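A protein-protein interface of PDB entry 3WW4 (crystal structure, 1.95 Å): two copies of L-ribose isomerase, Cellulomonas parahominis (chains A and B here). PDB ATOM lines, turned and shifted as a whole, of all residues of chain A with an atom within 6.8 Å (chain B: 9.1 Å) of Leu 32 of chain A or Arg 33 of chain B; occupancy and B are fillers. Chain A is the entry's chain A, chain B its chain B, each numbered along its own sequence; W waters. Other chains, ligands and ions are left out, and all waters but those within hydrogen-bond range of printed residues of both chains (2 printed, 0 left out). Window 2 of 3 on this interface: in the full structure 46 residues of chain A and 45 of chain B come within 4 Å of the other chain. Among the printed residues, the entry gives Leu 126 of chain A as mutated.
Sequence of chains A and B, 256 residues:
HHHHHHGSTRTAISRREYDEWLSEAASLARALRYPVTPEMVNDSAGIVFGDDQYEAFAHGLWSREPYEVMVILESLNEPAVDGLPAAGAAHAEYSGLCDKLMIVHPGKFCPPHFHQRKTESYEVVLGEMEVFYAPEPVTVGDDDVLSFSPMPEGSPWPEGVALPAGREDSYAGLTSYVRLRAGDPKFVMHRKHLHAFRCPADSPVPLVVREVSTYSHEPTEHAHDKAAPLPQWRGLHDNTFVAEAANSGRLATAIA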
ATOM      1  N   SER A  27     -20.190   3.589  12.233  1.00  0.00           N
ATOM      2  CA  SER A  27     -19.994   2.414  13.089  1.00  0.00           C
ATOM      3  C   SER A  27     -18.730   1.677  12.676  1.00  0.00           C
ATOM      4  O   SER A  27     -17.938   1.235  13.518  1.00  0.00           O
ATOM      5  CB  SER A  27     -21.177   1.451  12.976  1.00  0.00           C
ATOM      6  OG  SER A  27     -22.352   2.032  13.495  1.00  0.00           O
ATOM      7  N   LEU A  28     -18.555   1.538  11.368  1.00  0.00           N
ATOM      8  CA  LEU A  28     -17.395   0.866  10.821  1.00  0.00           C
ATOM      9  C   LEU A  28     -16.159   1.666  11.222  1.00  0.00           C
ATOM     10  O   LEU A  28     -15.136   1.097  11.604  1.00  0.00           O
ATOM     11  CB  LEU A  28     -17.532   0.774   9.294  1.00  0.00           C
ATOM     12  CG  LEU A  28     -16.580  -0.135   8.519  1.00  0.00           C
ATOM     13  CD1 LEU A  28     -16.623  -1.554   9.091  1.00  0.00           C
ATOM     14  CD2 LEU A  28     -16.973  -0.138   7.049  1.00  0.00           C
ATOM     15  N   ALA A  29     -16.264   2.992  11.155  1.00  0.00           N
ATOM     16  CA  ALA A  29     -15.156   3.864  11.538  1.00  0.00           C
ATOM     17  C   ALA A  29     -14.758   3.585  12.989  1.00  0.00           C
ATOM     18  O   ALA A  29     -13.592   3.322  13.290  1.00  0.00           O
ATOM     19  CB  ALA A  29     -15.564   5.325  11.384  1.00  0.00           C
ATOM     20  N   ARG A  30     -15.729   3.653  13.891  1.00  0.00           N
ATOM     21  CA  ARG A  30     -15.466   3.399  15.304  1.00  0.00           C
ATOM     22  C   ARG A  30     -14.855   2.019  15.514  1.00  0.00           C
ATOM     23  O   ARG A  30     -13.970   1.843  16.357  1.00  0.00           O
ATOM     24  CB  ARG A  30     -16.758   3.523  16.109  1.00  0.00           C
ATOM     25  CG  ARG A  30     -17.212   4.952  16.320  1.00  0.00           C
ATOM     26  CD  ARG A  30     -18.668   4.988  16.751  1.00  0.00           C
ATOM     27  NE  ARG A  30     -19.052   6.272  17.325  1.00  0.00           N
ATOM     28  CZ  ARG A  30     -18.681   6.692  18.530  1.00  0.00           C
ATOM     29  NH1 ARG A  30     -17.915   5.929  19.299  1.00  0.00           N
ATOM     30  NH2 ARG A  30     -19.074   7.879  18.964  1.00  0.00           N
ATOM     31  N   ALA A  31     -15.317   1.043  14.737  1.00  0.00           N
ATOM     32  CA  ALA A  31     -14.789  -0.313  14.837  1.00  0.00           C
ATOM     33  C   ALA A  31     -13.322  -0.297  14.445  1.00  0.00           C
ATOM     34  O   ALA A  31     -12.504  -1.049  14.981  1.00  0.00           O
ATOM     35  CB  ALA A  31     -15.557  -1.250  13.904  1.00  0.00           C
ATOM     36  N   LEU A  32     -12.991   0.565  13.494  1.00  0.00           N
ATOM     37  CA  LEU A  32     -11.623   0.649  13.029  1.00  0.00           C
ATOM     38  C   LEU A  32     -10.788   1.601  13.873  1.00  0.00           C
ATOM     39  O   LEU A  32      -9.673   1.955  13.499  1.00  0.00           O
ATOM     40  CB  LEU A  32     -11.609   1.053  11.553  1.00  0.00           C
ATOM     41  CG  LEU A  32     -12.242  -0.055  10.711  1.00  0.00           C
ATOM     42  CD1 LEU A  32     -12.603   0.459   9.329  1.00  0.00           C
ATOM     43  CD2 LEU A  32     -11.282  -1.231  10.633  1.00  0.00           C
ATOM     44  N   ARG A  33     -11.342   2.009  15.011  1.00  0.00           N
ATOM     45  CA  ARG A  33     -10.648   2.887  15.944  1.00  0.00           C
ATOM     46  C   ARG A  33     -10.509   4.359  15.538  1.00  0.00           C
ATOM     47  O   ARG A  33      -9.699   5.080  16.117  1.00  0.00           O
ATOM     48  CB  ARG A  33      -9.254   2.318  16.245  1.00  0.00           C
ATOM     49  CG  ARG A  33      -9.259   0.974  16.969  1.00  0.00           C
ATOM     50  CD  ARG A  33      -7.851   0.363  17.041  1.00  0.00           C
ATOM     51  NE  ARG A  33      -7.828  -0.853  17.853  1.00  0.00           N
ATOM     52  CZ  ARG A  33      -8.095  -0.874  19.153  1.00  0.00           C
ATOM     53  NH1 ARG A  33      -8.393   0.258  19.777  1.00  0.00           N
ATOM     54  NH2 ARG A  33      -8.085  -2.018  19.828  1.00  0.00           N
ATOM     55  N   TYR A  34     -11.277   4.821  14.559  1.00  0.00           N
ATOM     56  CA  TYR A  34     -11.175   6.229  14.164  1.00  0.00           C
ATOM     57  C   TYR A  34     -11.976   7.060  15.167  1.00  0.00           C
ATOM     58  O   TYR A  34     -13.049   6.654  15.594  1.00  0.00           O
ATOM     59  CB  TYR A  34     -11.733   6.437  12.750  1.00  0.00           C
ATOM     60  CG  TYR A  34     -11.311   7.743  12.102  1.00  0.00           C
ATOM     61  CD1 TYR A  34      -9.997   7.940  11.668  1.00  0.00           C
ATOM     62  CD2 TYR A  34     -12.219   8.784  11.935  1.00  0.00           C
ATOM     63  CE1 TYR A  34      -9.597   9.150  11.081  1.00  0.00           C
ATOM     64  CE2 TYR A  34     -11.834   9.990  11.354  1.00  0.00           C
ATOM     65  CZ  TYR A  34     -10.525  10.169  10.929  1.00  0.00           C
ATOM     66  OH  TYR A  34     -10.153  11.365  10.353  1.00  0.00           O
ATOM     67  N   LEU A 101     -11.669  10.104   7.403  1.00  0.00           N
ATOM     68  CA  LEU A 101     -11.812   8.698   7.069  1.00  0.00           C
ATOM     69  C   LEU A 101     -12.818   8.667   5.929  1.00  0.00           C
ATOM     70  O   LEU A 101     -13.896   9.262   6.026  1.00  0.00           O
ATOM     71  CB  LEU A 101     -12.328   7.909   8.274  1.00  0.00           C
ATOM     72  CG  LEU A 101     -12.057   6.405   8.198  1.00  0.00           C
ATOM     73  CD1 LEU A 101     -10.558   6.122   8.288  1.00  0.00           C
ATOM     74  CD2 LEU A 101     -12.807   5.712   9.325  1.00  0.00           C
ATOM     75  N   ILE A 103     -15.170   6.398   3.289  1.00  0.00           N
ATOM     76  CA  ILE A 103     -15.763   5.083   3.103  1.00  0.00           C
ATOM     77  C   ILE A 103     -16.441   5.027   1.743  1.00  0.00           C
ATOM     78  O   ILE A 103     -17.322   5.830   1.434  1.00  0.00           O
ATOM     79  CB  ILE A 103     -16.749   4.767   4.243  1.00  0.00           C
ATOM     80  CG1 ILE A 103     -16.037   4.970   5.584  1.00  0.00           C
ATOM     81  CG2 ILE A 103     -17.261   3.331   4.129  1.00  0.00           C
ATOM     82  CD1 ILE A 103     -16.909   4.764   6.785  1.00  0.00           C
ATOM     83  N   GLU A 123      -3.851   5.955   3.455  1.00  0.00           N
ATOM     84  CA  GLU A 123      -3.571   4.839   4.333  1.00  0.00           C
ATOM     85  C   GLU A 123      -4.829   3.978   4.268  1.00  0.00           C
ATOM     86  O   GLU A 123      -5.874   4.349   4.813  1.00  0.00           O
ATOM     87  CB  GLU A 123      -3.357   5.326   5.758  1.00  0.00           C
ATOM     88  CG  GLU A 123      -2.992   4.231   6.735  1.00  0.00           C
ATOM     89  CD  GLU A 123      -2.991   4.724   8.165  1.00  0.00           C
ATOM     90  OE1 GLU A 123      -2.334   5.751   8.443  1.00  0.00           O
ATOM     91  OE2 GLU A 123      -3.646   4.081   9.010  1.00  0.00           O
ATOM     92  N   VAL A 124      -4.749   2.847   3.578  1.00  0.00           N
ATOM     93  CA  VAL A 124      -5.906   1.965   3.478  1.00  0.00           C
ATOM     94  C   VAL A 124      -6.085   1.204   4.786  1.00  0.00           C
ATOM     95  O   VAL A 124      -5.161   0.539   5.261  1.00  0.00           O
ATOM     96  CB  VAL A 124      -5.751   0.968   2.316  1.00  0.00           C
ATOM     97  CG1 VAL A 124      -6.880  -0.085   2.365  1.00  0.00           C
ATOM     98  CG2 VAL A 124      -5.783   1.736   0.990  1.00  0.00           C
ATOM     99  N   VAL A 125      -7.278   1.302   5.365  1.00  0.00           N
ATOM    100  CA  VAL A 125      -7.559   0.631   6.626  1.00  0.00           C
ATOM    101  C   VAL A 125      -8.309  -0.683   6.423  1.00  0.00           C
ATOM    102  O   VAL A 125      -8.012  -1.684   7.073  1.00  0.00           O
ATOM    103  CB  VAL A 125      -8.371   1.561   7.562  1.00  0.00           C
ATOM    104  CG1 VAL A 125      -8.680   0.855   8.868  1.00  0.00           C
ATOM    105  CG2 VAL A 125      -7.580   2.832   7.831  1.00  0.00           C
ATOM    106  N   LEU A 126      -9.275  -0.680   5.512  1.00  0.00           N
ATOM    107  CA  LEU A 126     -10.067  -1.874   5.233  1.00  0.00           C
ATOM    108  C   LEU A 126     -10.329  -1.921   3.740  1.00  0.00           C
ATOM    109  O   LEU A 126     -10.538  -0.880   3.124  1.00  0.00           O
ATOM    110  CB  LEU A 126     -11.407  -1.810   5.984  1.00  0.00           C
ATOM    111  CG  LEU A 126     -12.223  -3.112   6.025  1.00  0.00           C
ATOM    112  CD1 LEU A 126     -11.621  -4.030   7.083  1.00  0.00           C
ATOM    113  CD2 LEU A 126     -13.691  -2.820   6.351  1.00  0.00           C
ATOM    114  N   ALA A 182      -4.119  -2.525   2.786  1.00  0.00           N
ATOM    115  CA  ALA A 182      -3.833  -2.191   4.170  1.00  0.00           C
ATOM    116  C   ALA A 182      -2.419  -2.654   4.484  1.00  0.00           C
ATOM    117  O   ALA A 182      -2.013  -3.750   4.085  1.00  0.00           O
ATOM    118  CB  ALA A 182      -4.825  -2.879   5.085  1.00  0.00           C
ATOM    119  N   GLY A 183      -1.665  -1.816   5.184  1.00  0.00           N
ATOM    120  CA  GLY A 183      -0.307  -2.171   5.545  1.00  0.00           C
ATOM    121  C   GLY A 183       0.720  -1.637   4.573  1.00  0.00           C
ATOM    122  O   GLY A 183       1.922  -1.682   4.851  1.00  0.00           O
ATOM    123  N   VAL A 208     -12.218   1.458   3.261  1.00  0.00           N
ATOM    124  CA  VAL A 208     -12.086   2.419   4.339  1.00  0.00           C
ATOM    125  C   VAL A 208     -10.656   2.920   4.303  1.00  0.00           C
ATOM    126  O   VAL A 208      -9.715   2.158   4.500  1.00  0.00           O
ATOM    127  CB  VAL A 208     -12.378   1.786   5.697  1.00  0.00           C
ATOM    128  CG1 VAL A 208     -12.314   2.855   6.779  1.00  0.00           C
ATOM    129  CG2 VAL A 208     -13.766   1.151   5.678  1.00  0.00           C
ATOM    130  N   ARG A 210      -7.856   6.213   5.358  1.00  0.00           N
ATOM    131  CA  ARG A 210      -7.584   7.437   6.087  1.00  0.00           C
ATOM    132  C   ARG A 210      -6.807   8.409   5.207  1.00  0.00           C
ATOM    133  O   ARG A 210      -5.760   8.072   4.638  1.00  0.00           O
ATOM    134  CB  ARG A 210      -6.771   7.170   7.360  1.00  0.00           C
ATOM    135  CG  ARG A 210      -6.463   8.461   8.139  1.00  0.00           C
ATOM    136  CD  ARG A 210      -5.521   8.258   9.321  1.00  0.00           C
ATOM    137  NE  ARG A 210      -6.052   7.324  10.317  1.00  0.00           N
ATOM    138  CZ  ARG A 210      -6.353   7.647  11.572  1.00  0.00           C
ATOM    139  NH1 ARG A 210      -6.827   6.724  12.396  1.00  0.00           N
ATOM    140  NH2 ARG A 210      -6.182   8.890  12.007  1.00  0.00           N
ATOM    141  N   ALA B  26       6.615  -2.743  17.213  1.00  0.00           N
ATOM    142  CA  ALA B  26       6.112  -2.880  15.853  1.00  0.00           C
ATOM    143  C   ALA B  26       4.916  -3.839  15.831  1.00  0.00           C
ATOM    144  O   ALA B  26       3.965  -3.629  15.084  1.00  0.00           O
ATOM    145  CB  ALA B  26       7.218  -3.390  14.927  1.00  0.00           C
ATOM    146  N   SER B  27       4.971  -4.886  16.655  1.00  0.00           N
ATOM    147  CA  SER B  27       3.889  -5.869  16.733  1.00  0.00           C
ATOM    148  C   SER B  27       2.629  -5.250  17.317  1.00  0.00           C
ATOM    149  O   SER B  27       1.523  -5.526  16.864  1.00  0.00           O
ATOM    150  CB  SER B  27       4.301  -7.060  17.606  1.00  0.00           C
ATOM    151  OG  SER B  27       5.476  -7.672  17.112  1.00  0.00           O
ATOM    152  N   LEU B  28       2.791  -4.433  18.345  1.00  0.00           N
ATOM    153  CA  LEU B  28       1.636  -3.799  18.945  1.00  0.00           C
ATOM    154  C   LEU B  28       1.048  -2.836  17.919  1.00  0.00           C
ATOM    155  O   LEU B  28      -0.174  -2.725  17.788  1.00  0.00           O
ATOM    156  CB  LEU B  28       2.030  -3.049  20.216  1.00  0.00           C
ATOM    157  CG  LEU B  28       0.880  -2.339  20.941  1.00  0.00           C
ATOM    158  CD1 LEU B  28      -0.150  -3.362  21.377  1.00  0.00           C
ATOM    159  CD2 LEU B  28       1.418  -1.579  22.147  1.00  0.00           C
ATOM    160  N   ALA B  29       1.927  -2.157  17.182  1.00  0.00           N
ATOM    161  CA  ALA B  29       1.501  -1.213  16.161  1.00  0.00           C
ATOM    162  C   ALA B  29       0.699  -1.934  15.086  1.00  0.00           C
ATOM    163  O   ALA B  29      -0.357  -1.462  14.662  1.00  0.00           O
ATOM    164  CB  ALA B  29       2.706  -0.541  15.534  1.00  0.00           C
ATOM    165  N   ARG B  30       1.206  -3.078  14.637  1.00  0.00           N
ATOM    166  CA  ARG B  30       0.506  -3.832  13.614  1.00  0.00           C
ATOM    167  C   ARG B  30      -0.826  -4.362  14.147  1.00  0.00           C
ATOM    168  O   ARG B  30      -1.824  -4.399  13.425  1.00  0.00           O
ATOM    169  CB  ARG B  30       1.381  -4.982  13.114  1.00  0.00           C
ATOM    170  CG  ARG B  30       2.593  -4.526  12.302  1.00  0.00           C
ATOM    171  CD  ARG B  30       3.331  -5.710  11.697  1.00  0.00           C
ATOM    172  NE  ARG B  30       4.690  -5.842  12.213  1.00  0.00           N
ATOM    173  CZ  ARG B  30       5.776  -5.412  11.580  1.00  0.00           C
ATOM    174  NH1 ARG B  30       5.668  -4.819  10.395  1.00  0.00           N
ATOM    175  NH2 ARG B  30       6.969  -5.570  12.134  1.00  0.00           N
ATOM    176  N   ALA B  31      -0.851  -4.766  15.412  1.00  0.00           N
ATOM    177  CA  ALA B  31      -2.085  -5.275  16.002  1.00  0.00           C
ATOM    178  C   ALA B  31      -3.152  -4.177  15.968  1.00  0.00           C
ATOM    179  O   ALA B  31      -4.343  -4.460  15.838  1.00  0.00           O
ATOM    180  CB  ALA B  31      -1.836  -5.728  17.442  1.00  0.00           C
ATOM    181  N   LEU B  32      -2.710  -2.925  16.080  1.00  0.00           N
ATOM    182  CA  LEU B  32      -3.609  -1.778  16.070  1.00  0.00           C
ATOM    183  C   LEU B  32      -3.828  -1.240  14.661  1.00  0.00           C
ATOM    184  O   LEU B  32      -4.377  -0.151  14.478  1.00  0.00           O
ATOM    185  CB  LEU B  32      -3.054  -0.678  16.978  1.00  0.00           C
ATOM    186  CG  LEU B  32      -3.126  -0.980  18.477  1.00  0.00           C
ATOM    187  CD1 LEU B  32      -2.334   0.045  19.267  1.00  0.00           C
ATOM    188  CD2 LEU B  32      -4.585  -0.976  18.908  1.00  0.00           C
ATOM    189  N   ARG B  33      -3.380  -2.009  13.675  1.00  0.00           N
ATOM    190  CA  ARG B  33      -3.533  -1.665  12.265  1.00  0.00           C
ATOM    191  C   ARG B  33      -2.704  -0.495  11.740  1.00  0.00           C
ATOM    192  O   ARG B  33      -3.026   0.040  10.684  1.00  0.00           O
ATOM    193  CB  ARG B  33      -5.005  -1.389  11.937  1.00  0.00           C
ATOM    194  CG  ARG B  33      -5.953  -2.584  12.066  1.00  0.00           C
ATOM    195  CD  ARG B  33      -7.389  -2.127  11.800  1.00  0.00           C
ATOM    196  NE  ARG B  33      -8.396  -3.173  11.985  1.00  0.00           N
ATOM    197  CZ  ARG B  33      -8.430  -4.309  11.300  1.00  0.00           C
ATOM    198  NH1 ARG B  33      -7.503  -4.552  10.381  1.00  0.00           N
ATOM    199  NH2 ARG B  33      -9.393  -5.198  11.522  1.00  0.00           N
ATOM    200  N   TYR B  34      -1.661  -0.071  12.448  1.00  0.00           N
ATOM    201  CA  TYR B  34      -0.857   1.021  11.910  1.00  0.00           C
ATOM    202  C   TYR B  34      -0.005   0.383  10.814  1.00  0.00           C
ATOM    203  O   TYR B  34       0.488  -0.733  10.971  1.00  0.00           O
ATOM    204  CB  TYR B  34       0.029   1.651  12.989  1.00  0.00           C
ATOM    205  CG  TYR B  34       0.626   2.991  12.585  1.00  0.00           C
ATOM    206  CD1 TYR B  34      -0.162   4.147  12.512  1.00  0.00           C
ATOM    207  CD2 TYR B  34       1.981   3.102  12.282  1.00  0.00           C
ATOM    208  CE1 TYR B  34       0.398   5.384  12.146  1.00  0.00           C
ATOM    209  CE2 TYR B  34       2.545   4.318  11.919  1.00  0.00           C
ATOM    210  CZ  TYR B  34       1.758   5.450  11.852  1.00  0.00           C
ATOM    211  OH  TYR B  34       2.350   6.639  11.485  1.00  0.00           O
ATOM    212  N   PRO B  35       0.170   1.074   9.682  1.00  0.00           N
ATOM    213  CA  PRO B  35       0.966   0.536   8.571  1.00  0.00           C
ATOM    214  C   PRO B  35       2.483   0.533   8.774  1.00  0.00           C
ATOM    215  O   PRO B  35       3.179   1.436   8.303  1.00  0.00           O
ATOM    216  CB  PRO B  35       0.531   1.409   7.397  1.00  0.00           C
ATOM    217  CG  PRO B  35       0.307   2.742   8.053  1.00  0.00           C
ATOM    218  CD  PRO B  35      -0.422   2.380   9.332  1.00  0.00           C
ATOM    219  N   VAL B  36       2.993  -0.489   9.462  1.00  0.00           N
ATOM    220  CA  VAL B  36       4.425  -0.600   9.720  1.00  0.00           C
ATOM    221  C   VAL B  36       5.152  -1.328   8.588  1.00  0.00           C
ATOM    222  O   VAL B  36       4.805  -2.456   8.244  1.00  0.00           O
ATOM    223  CB  VAL B  36       4.712  -1.359  11.051  1.00  0.00           C
ATOM    224  CG1 VAL B  36       6.208  -1.325  11.359  1.00  0.00           C
ATOM    225  CG2 VAL B  36       3.939  -0.735  12.196  1.00  0.00           C
ATOM    226  N   SER B  75       5.467   6.617   9.550  1.00  0.00           N
ATOM    227  CA  SER B  75       5.023   6.112   8.259  1.00  0.00           C
ATOM    228  C   SER B  75       4.995   7.215   7.202  1.00  0.00           C
ATOM    229  O   SER B  75       4.932   6.924   6.009  1.00  0.00           O
ATOM    230  CB  SER B  75       3.631   5.492   8.380  1.00  0.00           C
ATOM    231  OG  SER B  75       2.663   6.484   8.666  1.00  0.00           O
ATOM    232  N   LEU B 101       3.498   6.864  14.741  1.00  0.00           N
ATOM    233  CA  LEU B 101       2.894   6.208  15.893  1.00  0.00           C
ATOM    234  C   LEU B 101       3.950   6.251  16.990  1.00  0.00           C
ATOM    235  O   LEU B 101       5.110   5.880  16.772  1.00  0.00           O
ATOM    236  CB  LEU B 101       2.536   4.754  15.562  1.00  0.00           C
ATOM    237  CG  LEU B 101       1.519   4.147  16.533  1.00  0.00           C
ATOM    238  CD1 LEU B 101       0.177   4.871  16.350  1.00  0.00           C
ATOM    239  CD2 LEU B 101       1.360   2.640  16.290  1.00  0.00           C
ATOM    240  N   GLU B 123      -3.829  11.580  18.548  1.00  0.00           N
ATOM    241  CA  GLU B 123      -4.959  10.663  18.464  1.00  0.00           C
ATOM    242  C   GLU B 123      -4.548   9.446  19.270  1.00  0.00           C
ATOM    243  O   GLU B 123      -3.678   8.684  18.841  1.00  0.00           O
ATOM    244  CB  GLU B 123      -5.215  10.241  17.020  1.00  0.00           C
ATOM    245  CG  GLU B 123      -6.397   9.297  16.850  1.00  0.00           C
ATOM    246  CD  GLU B 123      -6.550   8.811  15.416  1.00  0.00           C
ATOM    247  OE1 GLU B 123      -6.570   9.653  14.496  1.00  0.00           O
ATOM    248  OE2 GLU B 123      -6.647   7.585  15.209  1.00  0.00           O
ATOM    249  N   VAL B 124      -5.153   9.264  20.437  1.00  0.00           N
ATOM    250  CA  VAL B 124      -4.801   8.125  21.273  1.00  0.00           C
ATOM    251  C   VAL B 124      -5.420   6.846  20.727  1.00  0.00           C
ATOM    252  O   VAL B 124      -6.626   6.779  20.476  1.00  0.00           O
ATOM    253  CB  VAL B 124      -5.234   8.362  22.726  1.00  0.00           C
ATOM    254  CG1 VAL B 124      -4.945   7.131  23.581  1.00  0.00           C
ATOM    255  CG2 VAL B 124      -4.494   9.581  23.278  1.00  0.00           C
ATOM    256  N   VAL B 125      -4.578   5.837  20.522  1.00  0.00           N
ATOM    257  CA  VAL B 125      -5.033   4.557  19.994  1.00  0.00           C
ATOM    258  C   VAL B 125      -5.256   3.530  21.102  1.00  0.00           C
ATOM    259  O   VAL B 125      -6.246   2.800  21.086  1.00  0.00           O
ATOM    260  CB  VAL B 125      -4.014   3.963  19.000  1.00  0.00           C
ATOM    261  CG1 VAL B 125      -4.593   2.699  18.354  1.00  0.00           C
ATOM    262  CG2 VAL B 125      -3.658   4.996  17.945  1.00  0.00           C
ATOM    263  N   VAL B 208      -0.174   4.256  23.148  1.00  0.00           N
ATOM    264  CA  VAL B 208       0.065   4.245  21.712  1.00  0.00           C
ATOM    265  C   VAL B 208      -0.704   5.420  21.149  1.00  0.00           C
ATOM    266  O   VAL B 208      -1.934   5.467  21.229  1.00  0.00           O
ATOM    267  CB  VAL B 208      -0.413   2.949  21.047  1.00  0.00           C
ATOM    268  CG1 VAL B 208      -0.177   3.032  19.536  1.00  0.00           C
ATOM    269  CG2 VAL B 208       0.335   1.766  21.630  1.00  0.00           C
ATOM    270  N   ARG B 210      -1.106   8.264  17.808  1.00  0.00           N
ATOM    271  CA  ARG B 210      -0.824   8.626  16.435  1.00  0.00           C
ATOM    272  C   ARG B 210      -0.656  10.139  16.358  1.00  0.00           C
ATOM    273  O   ARG B 210      -1.557  10.896  16.720  1.00  0.00           O
ATOM    274  CB  ARG B 210      -1.964   8.193  15.509  1.00  0.00           C
ATOM    275  CG  ARG B 210      -1.711   8.526  14.040  1.00  0.00           C
ATOM    276  CD  ARG B 210      -2.980   8.389  13.197  1.00  0.00           C
ATOM    277  NE  ARG B 210      -3.392   7.002  12.983  1.00  0.00           N
ATOM    278  CZ  ARG B 210      -3.063   6.276  11.918  1.00  0.00           C
ATOM    279  NH1 ARG B 210      -3.484   5.024  11.813  1.00  0.00           N
ATOM    280  NH2 ARG B 210      -2.315   6.803  10.957  1.00  0.00           N
HETATM  281  O   HOH W   1      -8.761   2.845  20.234  1.00  0.00           O
HETATM  282  O   HOH W   2      -6.681   5.466  16.683  1.00  0.00           O
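The guanidinium group (NH2) of Arg 210 of chain A is in salt-bridge range of the side-chain carboxylate (OE1) of Glu 123 of chain B (2.6 Å).
The guanidinium group (NH1) of Arg 210 of chain A lies close to the guanidinium group (NE) of Arg 210 of chain B (3.5 Å).
The side-chain carboxylate (OE1) of Glu 123 of chain A lies within salt-bridge range of the guanidinium group (NH2) of Arg 210 of chain B, 2.7 Å away.
O of Glu 123 of chain A lies within hydrogen-bond range of N of Arg 210 of chain A, at 2.8 Å.
N of Val 125 of chain B lies within hydrogen-bond range of O of Val 208 of chain B, 2.8 Å away.
OE2 of Glu 123 of chain B is in salt-bridge range of NE of Arg 210 of chain B, at 3.99 Å.
Arg 33 of chain B touches Leu 32 of chain A.
NE of Arg 33 of chain A touches CD2 of Leu 32 of chain B, at 3.4 Å.
NH1 of Arg 33 of chain A touches O of Val 125 of chain B, at 3.6 Å.
Glu 123 of chain A touches Pro 35 of chain B (OE2 to CD, 3.7 Å).
No residue of chain B comes within 4 Å of Ala 31 of chain A.
Leu 32 of chain A touches one residue of chain B.
Tyr 34 of chain A touches none of the printed residues of chain B.
Printed residues of chain A within 4 Å of Leu 32 of chain B: Arg 33.
Arg 33 of chain B touches one residue of chain A.
Tyr 34 of chain B touches none of the printed residues of chain A.
Of the printed residues of chain A, Pro 35 of chain B touches Glu 123.
Printed residues of chain A within 4 Å of Glu 123 of chain B: Arg 210.
Of the 18 printed residues of chain B, 6 touch a printed residue of chain A.
Of the 18 printed residues of chain A, 4 touch a printed residue of chain B.
Among the printed residues, Asp or Glu carboxylates within 4 Å of a Lys or Arg side-chain nitrogen of the other chain: Glu 123 of chain A with Arg 210 of chain B (2.7 Å) and Arg 210 of chain A with Glu 123 of chain B (2.6 Å).
Leu 32 of chain A touches Arg 33 of chain B, and with the chains exchanged Arg 33 of chain A touches Leu 32 of chain B.
Arg 33 of chain A touches Val 125 of chain B, but with the chains exchanged Val 125 of chain A does not touch Arg 33 of chain B (4.4 Å).
Glu 123 of chain A touches Arg 210 of chain B, and with the chains exchanged Arg 210 of chain A touches Glu 123 of chain B.
Arg 210 of chain A touches its own counterpart, Arg 210 of chain B.
Positions printed for both chains: 27, 28, 29, 30, 31, 32, 33, 34, 101, 123, 124, 125, 208 and 210.
Of the 7 pairs that touch across the chains among the printed residues, 5 have their exchanged pair printed and touching as well.
Water W2 lies within hydrogen-bond range of the side-chain carboxylate of Glu 123 of chain B and the backbone carbonyl oxygen of Arg 33 of chain A.
Water W1 bridges the guanidinium group of Arg 33 of chain A and the backbone carbonyl oxygen of Val 125 of chain B.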
